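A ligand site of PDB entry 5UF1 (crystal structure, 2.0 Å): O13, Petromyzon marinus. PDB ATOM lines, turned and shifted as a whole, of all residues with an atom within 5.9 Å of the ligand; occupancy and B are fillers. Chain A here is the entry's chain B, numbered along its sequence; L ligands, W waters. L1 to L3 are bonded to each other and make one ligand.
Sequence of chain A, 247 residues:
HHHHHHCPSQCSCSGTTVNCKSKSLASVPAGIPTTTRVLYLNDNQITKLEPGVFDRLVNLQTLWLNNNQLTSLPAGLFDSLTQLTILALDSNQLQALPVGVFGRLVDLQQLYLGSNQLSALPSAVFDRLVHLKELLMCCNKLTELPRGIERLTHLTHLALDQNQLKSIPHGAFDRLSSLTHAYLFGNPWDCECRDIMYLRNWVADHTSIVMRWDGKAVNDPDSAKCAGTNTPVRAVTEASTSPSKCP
The side-chain carboxylate of Asp 161 is in hydrogen-bond range of an oxygen (O2) of LG2 L2. The side-chain amide nitrogen of Gln 162 sits at hydrogen-bond distance from an oxygen (O1) of LG3 L3, at 2.9 Å. The side-chain carboxylate of Asp 90 sits at hydrogen-bond distance from a nitrogen (N1) of LIG L1 (3.0 Å).
N of Asp 161 lies within hydrogen-bond range of O of Tyr 183 (3.4 Å). O of Asp 161 lies within hydrogen-bond range of N of Cys 139 (2.9 Å). O of Gln 162 lies close to N of Cys 139 (3.4 Å). O of Phe 185 lies within hydrogen-bond range of N of Gln 162, 2.9 Å away. The backbone carbonyl oxygen (O) of Cys 138 is in hydrogen-bond range of the backbone NH (N) of Ser 115 (2.8 Å). The side-chain hydroxyl (OG) of Ser 115 lies close to the side-chain sulfur (SG) of Cys 139, 3.8 Å away. The backbone carbonyl oxygen of Ser 115 sits close to the backbone NH of Ser 91 (3.4 Å). The backbone carbonyl oxygen (O) of Tyr 183 lies within hydrogen-bond range of the backbone NH (N) of Leu 160 (3.0 Å).
CZ3 of Trp 64 touches C8 of LIG L1, at 3.8 Å. Ala 88 touches the ligand. Tyr 112 touches the ligand. OG of Ser 115 touches O4 of LG3 L3, at 3.7 Å. Leu 136 touches the ligand. CB of Cys 138 touches O3 of LG2 L2, at 3.4 Å. SG of Cys 139 touches C1 of LG3 L3, at 3.7 Å. CB of Ala 159 touches O3 of LG2 L2, at 3.6 Å. Tyr 183 touches the ligand. Phe 185 touches the ligand. CG of Trp 213 touches C3 of LG2 L2, at 3.7 Å. Of the 19 residues printed, 14 come within 4 Å of the ligand.
Water W7 lies within hydrogen-bond range of O5 of LG2 L2 (2.7 Å) and OH of Tyr 183 (2.7 Å). Water W6 bridges O5 of LIG L1 and NE1 of Trp 213. Water W5 bridges an oxygen (O6) of LIG L1 and the side-chain hydroxyl of Tyr 112. Water W8 lies within hydrogen-bond range of the side-chain hydroxyl of Ser 115 (2.7 Å), an oxygen (O4) of LG3 L3 (3.0 Å) and the side-chain sulfur of Cys 138 (3.4 Å). Water W2 bridges the backbone NH (N) of Cys 138 (3.1 Å) and an oxygen (O3) of LG2 L2 (3.2 Å). Water W4 bridges the side-chain hydroxyl of Ser 91 and the side-chain carboxylate of Asp 90.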
ATOM      1  N   TRP A  64      -1.583  17.090 -20.855  1.00  0.00           N
ATOM      2  CA  TRP A  64      -2.236  18.293 -20.349  1.00  0.00           C
ATOM      3  C   TRP A  64      -1.417  19.510 -20.786  1.00  0.00           C
ATOM      4  O   TRP A  64      -0.362  19.794 -20.222  1.00  0.00           O
ATOM      5  CB  TRP A  64      -2.366  18.200 -18.826  1.00  0.00           C
ATOM      6  CG  TRP A  64      -3.038  16.935 -18.406  1.00  0.00           C
ATOM      7  CD1 TRP A  64      -2.442  15.753 -18.081  1.00  0.00           C
ATOM      8  CD2 TRP A  64      -4.448  16.730 -18.223  1.00  0.00           C
ATOM      9  NE1 TRP A  64      -3.379  14.819 -17.737  1.00  0.00           N
ATOM     10  CE2 TRP A  64      -4.619  15.396 -17.803  1.00  0.00           C
ATOM     11  CE3 TRP A  64      -5.573  17.547 -18.365  1.00  0.00           C
ATOM     12  CZ2 TRP A  64      -5.881  14.860 -17.537  1.00  0.00           C
ATOM     13  CZ3 TRP A  64      -6.827  17.007 -18.102  1.00  0.00           C
ATOM     14  CH2 TRP A  64      -6.975  15.676 -17.691  1.00  0.00           C
ATOM     15  N   ASN A  66      -3.162  22.517 -21.126  1.00  0.00           N
ATOM     16  CA  ASN A  66      -4.075  23.600 -20.827  1.00  0.00           C
ATOM     17  C   ASN A  66      -3.371  24.734 -20.073  1.00  0.00           C
ATOM     18  O   ASN A  66      -2.312  24.545 -19.480  1.00  0.00           O
ATOM     19  CB  ASN A  66      -5.269  23.092 -20.020  1.00  0.00           C
ATOM     20  CG  ASN A  66      -4.868  22.019 -19.017  1.00  0.00           C
ATOM     21  OD1 ASN A  66      -4.087  21.116 -19.324  1.00  0.00           O
ATOM     22  ND2 ASN A  66      -5.421  22.106 -17.808  1.00  0.00           N
ATOM     23  N   ALA A  88      -5.669  17.876 -23.422  1.00  0.00           N
ATOM     24  CA  ALA A  88      -6.193  19.138 -22.915  1.00  0.00           C
ATOM     25  C   ALA A  88      -5.434  20.298 -23.562  1.00  0.00           C
ATOM     26  O   ALA A  88      -4.222  20.426 -23.386  1.00  0.00           O
ATOM     27  CB  ALA A  88      -6.078  19.209 -21.393  1.00  0.00           C
ATOM     28  N   ASP A  90      -7.266  23.472 -23.540  1.00  0.00           N
ATOM     29  CA  ASP A  90      -8.124  24.591 -23.173  1.00  0.00           C
ATOM     30  C   ASP A  90      -7.317  25.700 -22.496  1.00  0.00           C
ATOM     31  O   ASP A  90      -6.237  25.475 -21.955  1.00  0.00           O
ATOM     32  CB  ASP A  90      -9.263  24.123 -22.244  1.00  0.00           C
ATOM     33  CG  ASP A  90      -8.769  23.322 -21.066  1.00  0.00           C
ATOM     34  OD1 ASP A  90      -8.025  22.342 -21.296  1.00  0.00           O
ATOM     35  OD2 ASP A  90      -9.109  23.662 -19.917  1.00  0.00           O
ATOM     36  N   SER A  91      -7.872  26.917 -22.566  1.00  0.00           N
ATOM     37  CA  SER A  91      -7.279  28.096 -21.923  1.00  0.00           C
ATOM     38  C   SER A  91      -5.893  28.399 -22.486  1.00  0.00           C
ATOM     39  O   SER A  91      -4.978  28.776 -21.758  1.00  0.00           O
ATOM     40  CB  SER A  91      -7.232  27.936 -20.405  1.00  0.00           C
ATOM     41  OG  SER A  91      -8.529  28.071 -19.830  1.00  0.00           O
ATOM     42  N   TYR A 112     -10.248  18.685 -24.915  1.00  0.00           N
ATOM     43  CA  TYR A 112     -10.543  19.990 -24.338  1.00  0.00           C
ATOM     44  C   TYR A 112      -9.989  21.068 -25.260  1.00  0.00           C
ATOM     45  O   TYR A 112      -8.772  21.136 -25.470  1.00  0.00           O
ATOM     46  CB  TYR A 112      -9.948  20.120 -22.934  1.00  0.00           C
ATOM     47  CG  TYR A 112     -10.512  19.154 -21.913  1.00  0.00           C
ATOM     48  CD1 TYR A 112     -10.126  17.815 -21.896  1.00  0.00           C
ATOM     49  CD2 TYR A 112     -11.407  19.583 -20.941  1.00  0.00           C
ATOM     50  CE1 TYR A 112     -10.638  16.934 -20.959  1.00  0.00           C
ATOM     51  CE2 TYR A 112     -11.908  18.716 -19.993  1.00  0.00           C
ATOM     52  CZ  TYR A 112     -11.526  17.388 -20.005  1.00  0.00           C
ATOM     53  OH  TYR A 112     -12.041  16.524 -19.068  1.00  0.00           O
ATOM     54  N   SER A 115     -12.066  27.908 -24.227  1.00  0.00           N
ATOM     55  CA  SER A 115     -11.351  29.108 -23.776  1.00  0.00           C
ATOM     56  C   SER A 115     -10.124  29.389 -24.641  1.00  0.00           C
ATOM     57  O   SER A 115      -9.048  29.712 -24.147  1.00  0.00           O
ATOM     58  CB  SER A 115     -10.958  28.998 -22.302  1.00  0.00           C
ATOM     59  OG  SER A 115     -12.108  28.886 -21.479  1.00  0.00           O
ATOM     60  N   LEU A 136     -15.168  19.443 -25.496  1.00  0.00           N
ATOM     61  CA  LEU A 136     -15.393  20.618 -24.661  1.00  0.00           C
ATOM     62  C   LEU A 136     -14.805  21.831 -25.365  1.00  0.00           C
ATOM     63  O   LEU A 136     -13.589  21.972 -25.457  1.00  0.00           O
ATOM     64  CB  LEU A 136     -14.796  20.393 -23.276  1.00  0.00           C
ATOM     65  CG  LEU A 136     -15.422  19.097 -22.751  1.00  0.00           C
ATOM     66  CD1 LEU A 136     -14.384  18.177 -22.164  1.00  0.00           C
ATOM     67  CD2 LEU A 136     -16.514  19.375 -21.729  1.00  0.00           C
ATOM     68  N   CYS A 138     -16.134  25.347 -25.131  1.00  0.00           N
ATOM     69  CA  CYS A 138     -16.710  26.609 -24.702  1.00  0.00           C
ATOM     70  C   CYS A 138     -15.796  27.773 -25.060  1.00  0.00           C
ATOM     71  O   CYS A 138     -14.631  27.603 -25.417  1.00  0.00           O
ATOM     72  CB  CYS A 138     -16.934  26.638 -23.193  1.00  0.00           C
ATOM     73  SG  CYS A 138     -15.514  27.327 -22.237  1.00  0.00           S
ATOM     74  N   CYS A 139     -16.361  28.968 -24.959  1.00  0.00           N
ATOM     75  CA  CYS A 139     -15.577  30.190 -24.777  1.00  0.00           C
ATOM     76  C   CYS A 139     -14.620  30.422 -25.946  1.00  0.00           C
ATOM     77  O   CYS A 139     -13.482  30.872 -25.768  1.00  0.00           O
ATOM     78  CB  CYS A 139     -14.825  30.111 -23.449  1.00  0.00           C
ATOM     79  SG  CYS A 139     -15.816  29.352 -22.105  1.00  0.00           S
ATOM     80  N   HIS A 157     -20.514  14.259 -23.271  1.00  0.00           N
ATOM     81  CA  HIS A 157     -20.373  15.672 -22.940  1.00  0.00           C
ATOM     82  C   HIS A 157     -20.076  16.447 -24.208  1.00  0.00           C
ATOM     83  O   HIS A 157     -19.116  16.139 -24.921  1.00  0.00           O
ATOM     84  CB  HIS A 157     -19.253  15.897 -21.914  1.00  0.00           C
ATOM     85  CG  HIS A 157     -19.542  15.325 -20.565  1.00  0.00           C
ATOM     86  ND1 HIS A 157     -19.752  13.989 -20.350  1.00  0.00           N
ATOM     87  CD2 HIS A 157     -19.646  15.920 -19.348  1.00  0.00           C
ATOM     88  CE1 HIS A 157     -19.986  13.777 -19.064  1.00  0.00           C
ATOM     89  NE2 HIS A 157     -19.923  14.939 -18.437  1.00  0.00           N
ATOM     90  N   ALA A 159     -19.794  20.571 -25.035  1.00  0.00           N
ATOM     91  CA  ALA A 159     -19.823  21.932 -24.501  1.00  0.00           C
ATOM     92  C   ALA A 159     -19.608  22.915 -25.653  1.00  0.00           C
ATOM     93  O   ALA A 159     -18.508  22.985 -26.220  1.00  0.00           O
ATOM     94  CB  ALA A 159     -18.764  22.118 -23.420  1.00  0.00           C
ATOM     95  N   LEU A 160     -20.649  23.661 -25.983  1.00  0.00           N
ATOM     96  CA  LEU A 160     -20.583  24.690 -27.020  1.00  0.00           C
ATOM     97  C   LEU A 160     -20.901  26.079 -26.467  1.00  0.00           C
ATOM     98  O   LEU A 160     -21.121  27.010 -27.254  1.00  0.00           O
ATOM     99  CB  LEU A 160     -21.539  24.363 -28.166  1.00  0.00           C
ATOM    100  CG  LEU A 160     -21.273  23.058 -28.921  1.00  0.00           C
ATOM    101  CD1 LEU A 160     -22.456  22.722 -29.821  1.00  0.00           C
ATOM    102  CD2 LEU A 160     -19.994  23.152 -29.725  1.00  0.00           C
ATOM    103  N   ASP A 161     -20.923  26.234 -25.153  1.00  0.00           N
ATOM    104  CA  ASP A 161     -21.387  27.479 -24.554  1.00  0.00           C
ATOM    105  C   ASP A 161     -20.426  28.631 -24.831  1.00  0.00           C
ATOM    106  O   ASP A 161     -19.233  28.427 -25.061  1.00  0.00           O
ATOM    107  CB  ASP A 161     -21.582  27.302 -23.050  1.00  0.00           C
ATOM    108  CG  ASP A 161     -20.337  26.759 -22.364  1.00  0.00           C
ATOM    109  OD1 ASP A 161     -20.041  25.557 -22.537  1.00  0.00           O
ATOM    110  OD2 ASP A 161     -19.655  27.523 -21.643  1.00  0.00           O
ATOM    111  N   GLN A 162     -20.979  29.841 -24.818  1.00  0.00           N
ATOM    112  CA  GLN A 162     -20.204  31.080 -24.913  1.00  0.00           C
ATOM    113  C   GLN A 162     -19.400  31.152 -26.201  1.00  0.00           C
ATOM    114  O   GLN A 162     -18.216  31.490 -26.218  1.00  0.00           O
ATOM    115  CB  GLN A 162     -19.296  31.241 -23.683  1.00  0.00           C
ATOM    116  CG  GLN A 162     -20.073  31.265 -22.371  1.00  0.00           C
ATOM    117  CD  GLN A 162     -19.157  31.229 -21.153  1.00  0.00           C
ATOM    118  OE1 GLN A 162     -18.610  32.249 -20.759  1.00  0.00           O
ATOM    119  NE2 GLN A 162     -19.010  30.053 -20.557  1.00  0.00           N
ATOM    120  N   TYR A 183     -24.121  21.802 -23.321  1.00  0.00           N
ATOM    121  CA  TYR A 183     -23.997  23.199 -22.914  1.00  0.00           C
ATOM    122  C   TYR A 183     -24.238  24.089 -24.124  1.00  0.00           C
ATOM    123  O   TYR A 183     -23.496  24.006 -25.117  1.00  0.00           O
ATOM    124  CB  TYR A 183     -22.624  23.480 -22.298  1.00  0.00           C
ATOM    125  CG  TYR A 183     -22.319  22.634 -21.076  1.00  0.00           C
ATOM    126  CD1 TYR A 183     -21.724  21.391 -21.187  1.00  0.00           C
ATOM    127  CD2 TYR A 183     -22.625  23.106 -19.800  1.00  0.00           C
ATOM    128  CE1 TYR A 183     -21.435  20.627 -20.068  1.00  0.00           C
ATOM    129  CE2 TYR A 183     -22.345  22.345 -18.678  1.00  0.00           C
ATOM    130  CZ  TYR A 183     -21.754  21.114 -18.818  1.00  0.00           C
ATOM    131  OH  TYR A 183     -21.474  20.354 -17.696  1.00  0.00           O
ATOM    132  N   PHE A 185     -25.649  27.632 -23.534  1.00  0.00           N
ATOM    133  CA  PHE A 185     -25.864  29.016 -23.118  1.00  0.00           C
ATOM    134  C   PHE A 185     -24.767  29.919 -23.666  1.00  0.00           C
ATOM    135  O   PHE A 185     -23.750  29.469 -24.207  1.00  0.00           O
ATOM    136  CB  PHE A 185     -25.918  29.103 -21.593  1.00  0.00           C
ATOM    137  CG  PHE A 185     -24.619  28.789 -20.906  1.00  0.00           C
ATOM    138  CD1 PHE A 185     -24.295  27.498 -20.540  1.00  0.00           C
ATOM    139  CD2 PHE A 185     -23.707  29.806 -20.622  1.00  0.00           C
ATOM    140  CE1 PHE A 185     -23.098  27.205 -19.905  1.00  0.00           C
ATOM    141  CE2 PHE A 185     -22.509  29.519 -19.995  1.00  0.00           C
ATOM    142  CZ  PHE A 185     -22.205  28.219 -19.637  1.00  0.00           C
ATOM    143  N   TRP A 213     -23.711  26.352 -16.333  1.00  0.00           N
ATOM    144  CA  TRP A 213     -22.516  26.219 -15.513  1.00  0.00           C
ATOM    145  C   TRP A 213     -22.461  27.336 -14.480  1.00  0.00           C
ATOM    146  O   TRP A 213     -22.356  28.514 -14.847  1.00  0.00           O
ATOM    147  CB  TRP A 213     -21.249  26.226 -16.384  1.00  0.00           C
ATOM    148  CG  TRP A 213     -19.991  25.853 -15.657  1.00  0.00           C
ATOM    149  CD1 TRP A 213     -19.093  26.703 -15.097  1.00  0.00           C
ATOM    150  CD2 TRP A 213     -19.502  24.530 -15.445  1.00  0.00           C
ATOM    151  NE1 TRP A 213     -18.066  25.992 -14.527  1.00  0.00           N
ATOM    152  CE2 TRP A 213     -18.288  24.652 -14.732  1.00  0.00           C
ATOM    153  CE3 TRP A 213     -19.951  23.254 -15.776  1.00  0.00           C
ATOM    154  CZ2 TRP A 213     -17.532  23.544 -14.341  1.00  0.00           C
ATOM    155  CZ3 TRP A 213     -19.202  22.156 -15.390  1.00  0.00           C
ATOM    156  CH2 TRP A 213     -17.999  22.306 -14.682  1.00  0.00           C
ATOM    157  N   GLY A 215     -19.959  27.145 -11.833  1.00  0.00           N
ATOM    158  CA  GLY A 215     -18.891  26.414 -11.188  1.00  0.00           C
ATOM    159  C   GLY A 215     -19.013  24.919 -11.342  1.00  0.00           C
ATOM    160  O   GLY A 215     -18.035  24.201 -11.094  1.00  0.00           O
HETATM  161  C1  LIG L   1     -11.136  23.188 -16.194  1.00  0.00           C
HETATM  162  C2  LIG L   1     -11.648  22.312 -17.333  1.00  0.00           C
HETATM  163  C3  LIG L   1     -12.605  23.105 -18.227  1.00  0.00           C
HETATM  164  C4  LIG L   1     -13.710  23.740 -17.386  1.00  0.00           C
HETATM  165  C5  LIG L   1     -13.118  24.522 -16.214  1.00  0.00           C
HETATM  166  C6  LIG L   1     -14.155  25.036 -15.235  1.00  0.00           C
HETATM  167  C7  LIG L   1     -10.033  20.547 -17.901  1.00  0.00           C
HETATM  168  C8  LIG L   1      -8.872  20.166 -18.772  1.00  0.00           C
HETATM  169  N1  LIG L   1     -10.539  21.769 -18.103  1.00  0.00           N
HETATM  170  O1  LIG L   1     -10.305  22.455 -15.375  1.00  0.00           O
HETATM  171  O2  LIG L   1     -13.183  22.232 -19.189  1.00  0.00           O
HETATM  172  O3  LIG L   1     -14.404  24.518 -18.290  1.00  0.00           O
HETATM  173  O4  LIG L   1     -12.234  23.681 -15.449  1.00  0.00           O
HETATM  174  O5  LIG L   1     -13.647  26.106 -14.465  1.00  0.00           O
HETATM  175  O6  LIG L   1     -10.503  19.786 -17.059  1.00  0.00           O
HETATM  176  C1  LG2 L   2     -15.806  24.498 -18.230  1.00  0.00           C
HETATM  177  C2  LG2 L   2     -16.419  25.799 -18.780  1.00  0.00           C
HETATM  178  C3  LG2 L   2     -17.955  25.713 -18.727  1.00  0.00           C
HETATM  179  C4  LG2 L   2     -18.452  24.462 -19.458  1.00  0.00           C
HETATM  180  C5  LG2 L   2     -17.709  23.233 -18.921  1.00  0.00           C
HETATM  181  C6  LG2 L   2     -17.990  21.949 -19.665  1.00  0.00           C
HETATM  182  O1  LG2 L   2     -16.136  26.848 -17.938  1.00  0.00           O
HETATM  183  O2  LG2 L   2     -18.557  26.831 -19.367  1.00  0.00           O
HETATM  184  O3  LG2 L   2     -18.221  24.566 -20.852  1.00  0.00           O
HETATM  185  O4  LG2 L   2     -16.285  23.402 -18.980  1.00  0.00           O
HETATM  186  O5  LG2 L   2     -17.598  20.833 -18.885  1.00  0.00           O
HETATM  187  C1  LG3 L   3     -15.585  27.945 -18.670  1.00  0.00           C
HETATM  188  C2  LG3 L   3     -16.243  29.204 -18.096  1.00  0.00           C
HETATM  189  C3  LG3 L   3     -15.751  29.477 -16.665  1.00  0.00           C
HETATM  190  C4  LG3 L   3     -14.216  29.525 -16.633  1.00  0.00           C
HETATM  191  C5  LG3 L   3     -13.640  28.245 -17.265  1.00  0.00           C
HETATM  192  C6  LG3 L   3     -12.124  28.271 -17.415  1.00  0.00           C
HETATM  193  O1  LG3 L   3     -17.672  29.136 -18.137  1.00  0.00           O
HETATM  194  O2  LG3 L   3     -16.242  30.739 -16.231  1.00  0.00           O
HETATM  195  O3  LG3 L   3     -13.770  30.655 -17.371  1.00  0.00           O
HETATM  196  O4  LG3 L   3     -14.177  28.010 -18.582  1.00  0.00           O
HETATM  197  O   HOH W   1     -19.715  30.450 -16.588  1.00  0.00           O
HETATM  198  O   HOH W   2     -15.775  23.605 -22.613  1.00  0.00           O
HETATM  199  O   HOH W   3     -13.176  30.749 -19.987  1.00  0.00           O
HETATM  200  O   HOH W   4     -10.148  26.132 -19.321  1.00  0.00           O
HETATM  201  O   HOH W   5     -10.034  17.034 -16.466  1.00  0.00           O
HETATM  202  O   HOH W   6     -15.628  27.478 -13.260  1.00  0.00           O
HETATM  203  O   HOH W   7     -19.209  18.944 -17.933  1.00  0.00           O
HETATM  204  O   HOH W   8     -12.682  26.358 -20.570  1.00  0.00           O
HETATM  205  O   HOH W   9     -12.789  23.441 -21.796  1.00  0.00           O
HETATM  206  O   HOH W  10     -11.998  20.258 -14.222  1.00  0.00           O
HETATM  207  O   HOH W  11     -15.937  33.402 -17.329  1.00  0.00           O
HETATM  208  O   HOH W  12     -15.113  20.446 -18.089  1.00  0.00           O
